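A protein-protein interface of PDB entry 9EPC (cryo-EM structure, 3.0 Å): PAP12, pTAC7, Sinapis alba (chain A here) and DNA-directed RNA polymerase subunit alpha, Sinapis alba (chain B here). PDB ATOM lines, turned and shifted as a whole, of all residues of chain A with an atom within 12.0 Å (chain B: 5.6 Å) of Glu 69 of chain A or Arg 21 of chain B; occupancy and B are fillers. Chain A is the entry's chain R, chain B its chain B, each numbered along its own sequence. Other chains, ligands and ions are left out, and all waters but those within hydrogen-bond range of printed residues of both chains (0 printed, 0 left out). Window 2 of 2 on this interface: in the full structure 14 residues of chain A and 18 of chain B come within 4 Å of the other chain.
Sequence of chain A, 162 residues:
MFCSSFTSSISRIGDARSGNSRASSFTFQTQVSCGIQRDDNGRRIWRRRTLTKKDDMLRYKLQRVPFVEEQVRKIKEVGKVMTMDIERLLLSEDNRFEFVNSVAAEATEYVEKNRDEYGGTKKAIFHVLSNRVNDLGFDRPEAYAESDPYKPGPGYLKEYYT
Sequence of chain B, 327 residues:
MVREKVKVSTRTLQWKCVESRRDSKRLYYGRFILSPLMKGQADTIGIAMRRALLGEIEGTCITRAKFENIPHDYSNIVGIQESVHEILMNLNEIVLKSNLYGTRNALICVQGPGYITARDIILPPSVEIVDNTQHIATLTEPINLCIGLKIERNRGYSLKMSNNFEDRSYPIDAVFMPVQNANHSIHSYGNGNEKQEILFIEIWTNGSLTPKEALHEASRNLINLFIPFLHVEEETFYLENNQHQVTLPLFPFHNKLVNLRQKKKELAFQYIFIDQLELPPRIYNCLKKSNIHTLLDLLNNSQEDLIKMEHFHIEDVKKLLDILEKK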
ATOM      1  N   ARG A  64       6.760  11.120 -16.405  1.00  0.00           N
ATOM      2  CA  ARG A  64       7.485  10.895 -15.164  1.00  0.00           C
ATOM      3  C   ARG A  64       7.233   9.475 -14.683  1.00  0.00           C
ATOM      4  O   ARG A  64       6.101   8.984 -14.741  1.00  0.00           O
ATOM      5  CB  ARG A  64       7.063  11.900 -14.084  1.00  0.00           C
ATOM      6  CG  ARG A  64       5.559  12.096 -13.981  1.00  0.00           C
ATOM      7  CD  ARG A  64       5.185  13.009 -12.824  1.00  0.00           C
ATOM      8  NE  ARG A  64       5.367  12.361 -11.531  1.00  0.00           N
ATOM      9  CZ  ARG A  64       6.420  12.536 -10.745  1.00  0.00           C
ATOM     10  NH1 ARG A  64       7.411  13.342 -11.088  1.00  0.00           N
ATOM     11  NH2 ARG A  64       6.477  11.890  -9.585  1.00  0.00           N
ATOM     12  N   VAL A  65       8.290   8.817 -14.216  1.00  0.00           N
ATOM     13  CA  VAL A  65       8.186   7.440 -13.740  1.00  0.00           C
ATOM     14  C   VAL A  65       7.369   7.427 -12.452  1.00  0.00           C
ATOM     15  O   VAL A  65       7.434   8.381 -11.663  1.00  0.00           O
ATOM     16  CB  VAL A  65       9.572   6.810 -13.538  1.00  0.00           C
ATOM     17  CG1 VAL A  65      10.382   6.893 -14.824  1.00  0.00           C
ATOM     18  CG2 VAL A  65      10.300   7.487 -12.399  1.00  0.00           C
ATOM     19  N   PRO A  66       6.569   6.393 -12.215  1.00  0.00           N
ATOM     20  CA  PRO A  66       5.679   6.401 -11.050  1.00  0.00           C
ATOM     21  C   PRO A  66       6.193   5.636  -9.840  1.00  0.00           C
ATOM     22  O   PRO A  66       5.577   5.700  -8.773  1.00  0.00           O
ATOM     23  CB  PRO A  66       4.401   5.761 -11.604  1.00  0.00           C
ATOM     24  CG  PRO A  66       4.856   4.935 -12.810  1.00  0.00           C
ATOM     25  CD  PRO A  66       6.308   5.236 -13.084  1.00  0.00           C
ATOM     26  N   PHE A  67       7.305   4.914  -9.971  1.00  0.00           N
ATOM     27  CA  PHE A  67       7.688   3.977  -8.920  1.00  0.00           C
ATOM     28  C   PHE A  67       9.042   4.295  -8.301  1.00  0.00           C
ATOM     29  O   PHE A  67       9.866   3.395  -8.113  1.00  0.00           O
ATOM     30  CB  PHE A  67       7.701   2.549  -9.465  1.00  0.00           C
ATOM     31  CG  PHE A  67       6.405   2.125 -10.080  1.00  0.00           C
ATOM     32  CD1 PHE A  67       5.273   1.968  -9.303  1.00  0.00           C
ATOM     33  CD2 PHE A  67       6.318   1.874 -11.435  1.00  0.00           C
ATOM     34  CE1 PHE A  67       4.080   1.577  -9.868  1.00  0.00           C
ATOM     35  CE2 PHE A  67       5.127   1.481 -12.003  1.00  0.00           C
ATOM     36  CZ  PHE A  67       4.008   1.333 -11.219  1.00  0.00           C
ATOM     37  N   VAL A  68       9.282   5.560  -7.971  1.00  0.00           N
ATOM     38  CA  VAL A  68      10.531   5.958  -7.340  1.00  0.00           C
ATOM     39  C   VAL A  68      10.303   6.484  -5.924  1.00  0.00           C
ATOM     40  O   VAL A  68      11.159   7.163  -5.373  1.00  0.00           O
ATOM     41  CB  VAL A  68      11.284   6.986  -8.203  1.00  0.00           C
ATOM     42  CG1 VAL A  68      11.926   6.300  -9.391  1.00  0.00           C
ATOM     43  CG2 VAL A  68      10.336   8.075  -8.667  1.00  0.00           C
ATOM     44  N   GLU A  69       9.150   6.172  -5.329  1.00  0.00           N
ATOM     45  CA  GLU A  69       8.872   6.637  -3.974  1.00  0.00           C
ATOM     46  C   GLU A  69       9.862   6.055  -2.976  1.00  0.00           C
ATOM     47  O   GLU A  69      10.311   6.750  -2.057  1.00  0.00           O
ATOM     48  CB  GLU A  69       7.441   6.279  -3.573  1.00  0.00           C
ATOM     49  CG  GLU A  69       6.366   7.095  -4.265  1.00  0.00           C
ATOM     50  CD  GLU A  69       6.123   6.662  -5.695  1.00  0.00           C
ATOM     51  OE1 GLU A  69       6.714   5.648  -6.121  1.00  0.00           O
ATOM     52  OE2 GLU A  69       5.338   7.334  -6.394  1.00  0.00           O
ATOM     53  N   GLU A  70      10.207   4.777  -3.131  1.00  0.00           N
ATOM     54  CA  GLU A  70      11.158   4.159  -2.216  1.00  0.00           C
ATOM     55  C   GLU A  70      12.578   4.650  -2.462  1.00  0.00           C
ATOM     56  O   GLU A  70      13.380   4.712  -1.524  1.00  0.00           O
ATOM     57  CB  GLU A  70      11.090   2.635  -2.333  1.00  0.00           C
ATOM     58  CG  GLU A  70      11.450   2.074  -3.705  1.00  0.00           C
ATOM     59  CD  GLU A  70      10.309   2.157  -4.707  1.00  0.00           C
ATOM     60  OE1 GLU A  70       9.699   3.238  -4.841  1.00  0.00           O
ATOM     61  OE2 GLU A  70      10.020   1.132  -5.361  1.00  0.00           O
ATOM     62  N   GLN A  71      12.912   4.994  -3.708  1.00  0.00           N
ATOM     63  CA  GLN A  71      14.245   5.514  -3.993  1.00  0.00           C
ATOM     64  C   GLN A  71      14.435   6.901  -3.397  1.00  0.00           C
ATOM     65  O   GLN A  71      15.441   7.166  -2.727  1.00  0.00           O
ATOM     66  CB  GLN A  71      14.492   5.545  -5.499  1.00  0.00           C
ATOM     67  CG  GLN A  71      14.777   4.193  -6.114  1.00  0.00           C
ATOM     68  CD  GLN A  71      15.273   4.310  -7.536  1.00  0.00           C
ATOM     69  OE1 GLN A  71      15.481   5.411  -8.040  1.00  0.00           O
ATOM     70  NE2 GLN A  71      15.466   3.174  -8.191  1.00  0.00           N
ATOM     71  N   VAL A  72      13.477   7.802  -3.624  1.00  0.00           N
ATOM     72  CA  VAL A  72      13.631   9.173  -3.147  1.00  0.00           C
ATOM     73  C   VAL A  72      13.656   9.208  -1.624  1.00  0.00           C
ATOM     74  O   VAL A  72      14.374  10.014  -1.022  1.00  0.00           O
ATOM     75  CB  VAL A  72      12.529  10.078  -3.727  1.00  0.00           C
ATOM     76  CG1 VAL A  72      12.592  10.077  -5.241  1.00  0.00           C
ATOM     77  CG2 VAL A  72      11.154   9.642  -3.256  1.00  0.00           C
ATOM     78  N   ARG A  73      12.878   8.339  -0.978  1.00  0.00           N
ATOM     79  CA  ARG A  73      12.923   8.255   0.477  1.00  0.00           C
ATOM     80  C   ARG A  73      14.262   7.712   0.954  1.00  0.00           C
ATOM     81  O   ARG A  73      14.816   8.195   1.948  1.00  0.00           O
ATOM     82  CB  ARG A  73      11.776   7.386   0.985  1.00  0.00           C
ATOM     83  CG  ARG A  73      11.757   7.213   2.489  1.00  0.00           C
ATOM     84  CD  ARG A  73      10.562   6.395   2.937  1.00  0.00           C
ATOM     85  NE  ARG A  73      10.592   5.038   2.405  1.00  0.00           N
ATOM     86  CZ  ARG A  73       9.878   4.622   1.367  1.00  0.00           C
ATOM     87  NH1 ARG A  73       9.053   5.435   0.726  1.00  0.00           N
ATOM     88  NH2 ARG A  73       9.995   3.361   0.964  1.00  0.00           N
ATOM     89  N   LYS A  74      14.793   6.703   0.263  1.00  0.00           N
ATOM     90  CA  LYS A  74      16.090   6.150   0.637  1.00  0.00           C
ATOM     91  C   LYS A  74      17.202   7.172   0.447  1.00  0.00           C
ATOM     92  O   LYS A  74      18.104   7.277   1.285  1.00  0.00           O
ATOM     93  CB  LYS A  74      16.375   4.890  -0.177  1.00  0.00           C
ATOM     94  CG  LYS A  74      17.632   4.150   0.238  1.00  0.00           C
ATOM     95  CD  LYS A  74      17.509   3.609   1.651  1.00  0.00           C
ATOM     96  CE  LYS A  74      18.710   2.755   2.025  1.00  0.00           C
ATOM     97  NZ  LYS A  74      18.850   1.570   1.134  1.00  0.00           N
ATOM     98  N   ILE A  75      17.153   7.935  -0.647  1.00  0.00           N
ATOM     99  CA  ILE A  75      18.205   8.909  -0.931  1.00  0.00           C
ATOM    100  C   ILE A  75      18.264   9.963   0.166  1.00  0.00           C
ATOM    101  O   ILE A  75      19.342  10.309   0.663  1.00  0.00           O
ATOM    102  CB  ILE A  75      17.984   9.548  -2.313  1.00  0.00           C
ATOM    103  CG1 ILE A  75      18.217   8.525  -3.421  1.00  0.00           C
ATOM    104  CG2 ILE A  75      18.897  10.742  -2.502  1.00  0.00           C
ATOM    105  CD1 ILE A  75      17.904   9.054  -4.795  1.00  0.00           C
ATOM    106  N   LYS A  76      17.104  10.491   0.561  1.00  0.00           N
ATOM    107  CA  LYS A  76      17.076  11.491   1.622  1.00  0.00           C
ATOM    108  C   LYS A  76      17.566  10.909   2.941  1.00  0.00           C
ATOM    109  O   LYS A  76      18.339  11.550   3.662  1.00  0.00           O
ATOM    110  CB  LYS A  76      15.666  12.053   1.775  1.00  0.00           C
ATOM    111  CG  LYS A  76      15.138  12.744   0.535  1.00  0.00           C
ATOM    112  CD  LYS A  76      13.741  13.282   0.767  1.00  0.00           C
ATOM    113  CE  LYS A  76      13.204  13.961  -0.475  1.00  0.00           C
ATOM    114  NZ  LYS A  76      13.153  13.023  -1.626  1.00  0.00           N
ATOM    115  N   GLU A  77      17.126   9.694   3.273  1.00  0.00           N
ATOM    116  CA  GLU A  77      17.539   9.075   4.527  1.00  0.00           C
ATOM    117  C   GLU A  77      19.030   8.765   4.529  1.00  0.00           C
ATOM    118  O   GLU A  77      19.711   8.972   5.541  1.00  0.00           O
ATOM    119  CB  GLU A  77      16.724   7.807   4.775  1.00  0.00           C
ATOM    120  CG  GLU A  77      17.023   7.126   6.097  1.00  0.00           C
ATOM    121  CD  GLU A  77      16.075   5.979   6.386  1.00  0.00           C
ATOM    122  OE1 GLU A  77      15.197   5.705   5.541  1.00  0.00           O
ATOM    123  OE2 GLU A  77      16.206   5.354   7.459  1.00  0.00           O
ATOM    124  N   VAL A  78      19.554   8.264   3.410  1.00  0.00           N
ATOM    125  CA  VAL A  78      20.980   7.967   3.325  1.00  0.00           C
ATOM    126  C   VAL A  78      21.801   9.246   3.424  1.00  0.00           C
ATOM    127  O   VAL A  78      22.802   9.302   4.148  1.00  0.00           O
ATOM    128  CB  VAL A  78      21.285   7.195   2.030  1.00  0.00           C
ATOM    129  CG1 VAL A  78      22.768   7.239   1.721  1.00  0.00           C
ATOM    130  CG2 VAL A  78      20.817   5.758   2.156  1.00  0.00           C
ATOM    131  N   GLU A 146      17.677  15.073   9.905  1.00  0.00           N
ATOM    132  CA  GLU A 146      16.429  14.335   9.803  1.00  0.00           C
ATOM    133  C   GLU A 146      16.213  13.526  11.071  1.00  0.00           C
ATOM    134  O   GLU A 146      17.160  12.964  11.629  1.00  0.00           O
ATOM    135  CB  GLU A 146      16.426  13.402   8.587  1.00  0.00           C
ATOM    136  CG  GLU A 146      15.091  12.721   8.338  1.00  0.00           C
ATOM    137  CD  GLU A 146      15.220  11.492   7.462  1.00  0.00           C
ATOM    138  OE1 GLU A 146      16.357  11.016   7.269  1.00  0.00           O
ATOM    139  OE2 GLU A 146      14.184  11.002   6.969  1.00  0.00           O
ATOM    140  N   TYR A 150       9.307   7.120  13.105  1.00  0.00           N
ATOM    141  CA  TYR A 150       8.819   5.805  13.491  1.00  0.00           C
ATOM    142  C   TYR A 150       9.581   5.219  14.669  1.00  0.00           C
ATOM    143  O   TYR A 150       9.431   4.029  14.961  1.00  0.00           O
ATOM    144  CB  TYR A 150       8.881   4.859  12.294  1.00  0.00           C
ATOM    145  CG  TYR A 150       8.394   5.503  11.021  1.00  0.00           C
ATOM    146  CD1 TYR A 150       7.048   5.783  10.835  1.00  0.00           C
ATOM    147  CD2 TYR A 150       9.280   5.845  10.010  1.00  0.00           C
ATOM    148  CE1 TYR A 150       6.598   6.377   9.677  1.00  0.00           C
ATOM    149  CE2 TYR A 150       8.838   6.440   8.846  1.00  0.00           C
ATOM    150  CZ  TYR A 150       7.495   6.704   8.685  1.00  0.00           C
ATOM    151  OH  TYR A 150       7.049   7.297   7.528  1.00  0.00           O
ATOM    152  N   GLU B  19       1.837   7.116   4.434  1.00  0.00           N
ATOM    153  CA  GLU B  19       1.883   7.889   3.203  1.00  0.00           C
ATOM    154  C   GLU B  19       0.745   7.459   2.295  1.00  0.00           C
ATOM    155  O   GLU B  19       0.400   6.277   2.233  1.00  0.00           O
ATOM    156  CB  GLU B  19       3.220   7.715   2.475  1.00  0.00           C
ATOM    157  CG  GLU B  19       4.436   8.065   3.313  1.00  0.00           C
ATOM    158  CD  GLU B  19       5.733   7.957   2.534  1.00  0.00           C
ATOM    159  OE1 GLU B  19       5.719   8.217   1.313  1.00  0.00           O
ATOM    160  OE2 GLU B  19       6.766   7.608   3.143  1.00  0.00           O
ATOM    161  N   SER B  20       0.165   8.426   1.591  1.00  0.00           N
ATOM    162  CA  SER B  20      -0.937   8.151   0.674  1.00  0.00           C
ATOM    163  C   SER B  20      -0.943   9.243  -0.382  1.00  0.00           C
ATOM    164  O   SER B  20      -1.228  10.403  -0.073  1.00  0.00           O
ATOM    165  CB  SER B  20      -2.268   8.096   1.415  1.00  0.00           C
ATOM    166  OG  SER B  20      -3.342   7.917   0.511  1.00  0.00           O
ATOM    167  N   ARG B  21      -0.629   8.878  -1.621  1.00  0.00           N
ATOM    168  CA  ARG B  21      -0.569   9.828  -2.718  1.00  0.00           C
ATOM    169  C   ARG B  21      -1.415   9.325  -3.877  1.00  0.00           C
ATOM    170  O   ARG B  21      -1.583   8.120  -4.070  1.00  0.00           O
ATOM    171  CB  ARG B  21       0.869  10.059  -3.184  1.00  0.00           C
ATOM    172  CG  ARG B  21       1.845  10.359  -2.060  1.00  0.00           C
ATOM    173  CD  ARG B  21       3.185  10.853  -2.586  1.00  0.00           C
ATOM    174  NE  ARG B  21       3.763   9.957  -3.581  1.00  0.00           N
ATOM    175  CZ  ARG B  21       3.704  10.156  -4.891  1.00  0.00           C
ATOM    176  NH1 ARG B  21       3.095  11.214  -5.402  1.00  0.00           N
ATOM    177  NH2 ARG B  21       4.267   9.271  -5.708  1.00  0.00           N
ATOM    178  N   ARG B  22      -1.945  10.269  -4.646  1.00  0.00           N
ATOM    179  CA  ARG B  22      -2.848   9.995  -5.758  1.00  0.00           C
ATOM    180  C   ARG B  22      -2.447  10.818  -6.976  1.00  0.00           C
ATOM    181  O   ARG B  22      -3.254  11.535  -7.570  1.00  0.00           O
ATOM    182  CB  ARG B  22      -4.291  10.279  -5.352  1.00  0.00           C
ATOM    183  CG  ARG B  22      -5.335   9.740  -6.314  1.00  0.00           C
ATOM    184  CD  ARG B  22      -6.587  10.600  -6.304  1.00  0.00           C
ATOM    185  NE  ARG B  22      -7.537  10.194  -7.331  1.00  0.00           N
ATOM    186  CZ  ARG B  22      -7.501  10.608  -8.590  1.00  0.00           C
ATOM    187  NH1 ARG B  22      -6.561  11.435  -9.019  1.00  0.00           N
ATOM    188  NH2 ARG B  22      -8.427  10.178  -9.442  1.00  0.00           N
ATOM    189  N   ASP B  23      -1.175  10.742  -7.362  1.00  0.00           N
ATOM    190  CA  ASP B  23      -0.700  11.597  -8.441  1.00  0.00           C
ATOM    191  C   ASP B  23      -1.042  11.030  -9.812  1.00  0.00           C
ATOM    192  O   ASP B  23      -0.189  10.998 -10.704  1.00  0.00           O
ATOM    193  CB  ASP B  23       0.812  11.795  -8.332  1.00  0.00           C
ATOM    194  CG  ASP B  23       1.561  10.481  -8.238  1.00  0.00           C
ATOM    195  OD1 ASP B  23       1.440   9.800  -7.200  1.00  0.00           O
ATOM    196  OD2 ASP B  23       2.257  10.122  -9.210  1.00  0.00           O
ATOM    197  N   LEU B  27      -2.893   5.762 -10.863  1.00  0.00           N
ATOM    198  CA  LEU B  27      -1.651   5.476 -10.152  1.00  0.00           C
ATOM    199  C   LEU B  27      -1.818   5.984  -8.721  1.00  0.00           C
ATOM    200  O   LEU B  27      -1.689   7.185  -8.472  1.00  0.00           O
ATOM    201  CB  LEU B  27      -0.463   6.124 -10.843  1.00  0.00           C
ATOM    202  CG  LEU B  27       0.923   5.512 -10.624  1.00  0.00           C
ATOM    203  CD1 LEU B  27       1.479   5.835  -9.245  1.00  0.00           C
ATOM    204  CD2 LEU B  27       0.879   4.011 -10.846  1.00  0.00           C
ATOM    205  N   TYR B  28      -2.097   5.067  -7.801  1.00  0.00           N
ATOM    206  CA  TYR B  28      -2.248   5.391  -6.391  1.00  0.00           C
ATOM    207  C   TYR B  28      -1.068   4.819  -5.623  1.00  0.00           C
ATOM    208  O   TYR B  28      -0.575   3.733  -5.941  1.00  0.00           O
ATOM    209  CB  TYR B  28      -3.551   4.833  -5.814  1.00  0.00           C
ATOM    210  CG  TYR B  28      -4.823   5.481  -6.316  1.00  0.00           C
ATOM    211  CD1 TYR B  28      -4.842   6.227  -7.485  1.00  0.00           C
ATOM    212  CD2 TYR B  28      -6.009   5.350  -5.610  1.00  0.00           C
ATOM    213  CE1 TYR B  28      -6.003   6.811  -7.941  1.00  0.00           C
ATOM    214  CE2 TYR B  28      -7.174   5.936  -6.056  1.00  0.00           C
ATOM    215  CZ  TYR B  28      -7.165   6.667  -7.222  1.00  0.00           C
ATOM    216  OH  TYR B  28      -8.324   7.252  -7.673  1.00  0.00           O
ATOM    217  N   TYR B  29      -0.614   5.553  -4.615  1.00  0.00           N
ATOM    218  CA  TYR B  29       0.503   5.130  -3.789  1.00  0.00           C
ATOM    219  C   TYR B  29       0.075   5.107  -2.332  1.00  0.00           C
ATOM    220  O   TYR B  29      -0.711   5.951  -1.894  1.00  0.00           O
ATOM    221  CB  TYR B  29       1.706   6.052  -3.965  1.00  0.00           C
ATOM    222  CG  TYR B  29       2.823   5.778  -2.994  1.00  0.00           C
ATOM    223  CD1 TYR B  29       3.656   4.684  -3.158  1.00  0.00           C
ATOM    224  CD2 TYR B  29       3.049   6.616  -1.915  1.00  0.00           C
ATOM    225  CE1 TYR B  29       4.675   4.432  -2.277  1.00  0.00           C
ATOM    226  CE2 TYR B  29       4.068   6.369  -1.027  1.00  0.00           C
ATOM    227  CZ  TYR B  29       4.879   5.276  -1.212  1.00  0.00           C
ATOM    228  OH  TYR B  29       5.900   5.027  -0.327  1.00  0.00           O
ATOM    229  N   GLY B  30       0.588   4.134  -1.589  1.00  0.00           N
ATOM    230  CA  GLY B  30       0.286   4.025  -0.178  1.00  0.00           C
ATOM    231  C   GLY B  30       1.358   3.285   0.589  1.00  0.00           C
ATOM    232  O   GLY B  30       1.816   2.224   0.157  1.00  0.00           O
ATOM    233  N   GLU B 202       4.551  -1.166   1.124  1.00  0.00           N
ATOM    234  CA  GLU B 202       4.480  -0.117   0.113  1.00  0.00           C
ATOM    235  C   GLU B 202       3.721  -0.672  -1.081  1.00  0.00           C
ATOM    236  O   GLU B 202       4.155  -1.657  -1.684  1.00  0.00           O
ATOM    237  CB  GLU B 202       5.880   0.341  -0.287  1.00  0.00           C
ATOM    238  CG  GLU B 202       6.004   1.824  -0.513  1.00  0.00           C
ATOM    239  CD  GLU B 202       7.443   2.287  -0.513  1.00  0.00           C
ATOM    240  OE1 GLU B 202       8.335   1.452  -0.260  1.00  0.00           O
ATOM    241  OE2 GLU B 202       7.682   3.487  -0.761  1.00  0.00           O
ATOM    242  N   TRP B 204       1.573   0.076  -4.754  1.00  0.00           N
ATOM    243  CA  TRP B 204       1.184   0.890  -5.896  1.00  0.00           C
ATOM    244  C   TRP B 204       0.029   0.208  -6.612  1.00  0.00           C
ATOM    245  O   TRP B 204       0.141  -0.956  -7.002  1.00  0.00           O
ATOM    246  CB  TRP B 204       2.346   1.079  -6.872  1.00  0.00           C
ATOM    247  CG  TRP B 204       3.442   1.953  -6.379  1.00  0.00           C
ATOM    248  CD1 TRP B 204       3.566   3.294  -6.571  1.00  0.00           C
ATOM    249  CD2 TRP B 204       4.589   1.545  -5.630  1.00  0.00           C
ATOM    250  NE1 TRP B 204       4.716   3.750  -5.981  1.00  0.00           N
ATOM    251  CE2 TRP B 204       5.362   2.694  -5.395  1.00  0.00           C
ATOM    252  CE3 TRP B 204       5.034   0.319  -5.131  1.00  0.00           C
ATOM    253  CZ2 TRP B 204       6.553   2.656  -4.682  1.00  0.00           C
ATOM    254  CZ3 TRP B 204       6.215   0.284  -4.425  1.00  0.00           C
ATOM    255  CH2 TRP B 204       6.962   1.443  -4.206  1.00  0.00           C
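Of the 17 printed residues of chain A, 5 touch a printed residue of chain B. Printed residues of chain A that touch a printed residue of chain B: Pro 66, Phe 67, Glu 69, Glu 70 and Arg 73. Printed residues of chain B that touch a printed residue of chain A: Glu 19, Arg 21, Leu 27, Tyr 29, Glu 202 and Trp 204. Among the printed residues, 12 pairs touch across the chains. Among the printed residues, Asp or Glu carboxylates within 4 Å of a Lys or Arg side-chain nitrogen of the other chain: Glu 69 of chain A with Arg 21 of chain B, Arg 73 of chain A with Glu 19 of chain B and Arg 73 of chain A with Glu 202 of chain B.
NH1 of Arg 73 of chain A is in hydrogen-bond range of O of Glu 69 of chain A, at 3.3 Å. The backbone carbonyl oxygen of Arg 21 of chain B lies within hydrogen-bond range of the backbone NH of Tyr 29 of chain B. The guanidinium group (NH1) of Arg 21 of chain B lies within salt-bridge range of the side-chain carboxylate (OD1) of Asp 23 of chain B (2.8 Å).
OH of Tyr 29 of chain B sits at hydrogen-bond distance from NH1 of Arg 73 of chain A, at 3.3 Å. The side-chain carboxylate of Glu 202 of chain B is in salt-bridge range of the guanidinium group of Arg 73 of chain A, 2.8 Å away. NE1 of Trp 204 of chain B sits at hydrogen-bond distance from OE1 of Glu 69 of chain A (2.8 Å). The side-chain carboxylate of Glu 19 of chain B is in salt-bridge range of the guanidinium group of Arg 73 of chain A (3.97 Å). NH2 of Arg 21 of chain B sits close to OE2 of Glu 69 of chain A (2.3 Å).
Among the printed residues, pairs that only touch across the chains: Pro 66 of chain A with Leu 27 of chain B (3.6 Å), Pro 66 of chain A with Trp 204 of chain B (3.5 Å), Phe 67 of chain A with Trp 204 of chain B (3.5 Å), Glu 69 of chain A with Tyr 29 of chain B (3.6 Å), Glu 69 of chain A with Glu 202 of chain B (3.97 Å), Glu 70 of chain A with Glu 202 of chain B (3.6 Å) and Glu 70 of chain A with Trp 204 of chain B (3.2 Å).
Printed residues of chain B within 4 Å of Phe 67 of chain A: Trp 204 (3.5 Å). Of chain B, only Arg 21, Tyr 29, Glu 202 and Trp 204 come within 4 Å of Glu 69 of chain A. Lys 76 of chain A touches none of the printed residues of chain B. Glu 77 of chain A touches none of the printed residues of chain B. Of chain A, only Glu 69 (2.3 Å) comes within 4 Å of Arg 21 of chain B. No residue of chain A comes within 4 Å of Asp 23 of chain B. Leu 27 of chain B touches one residue of chain A. Of chain A, only Glu 69 and Arg 73 come within 4 Å of Tyr 29 of chain B. Of the printed residues of chain A, Glu 202 of chain B touches Glu 69, Glu 70 and Arg 73. Of the printed residues of chain A, Trp 204 of chain B touches Pro 66 (3.5 Å), Phe 67 (3.5 Å), Glu 69 (2.8 Å) and Glu 70 (3.2 Å). The nearest residue of chain B that does not touch Glu 69 of chain A is Asp 23 of chain B (4.7 Å). The nearest residue of chain A that does not touch Arg 21 of chain B is Pro 66 of chain A (4.9 Å). The nearest printed residue of chain B that does not touch Arg 73 of chain A is Trp 204 of chain B (6.3 Å).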
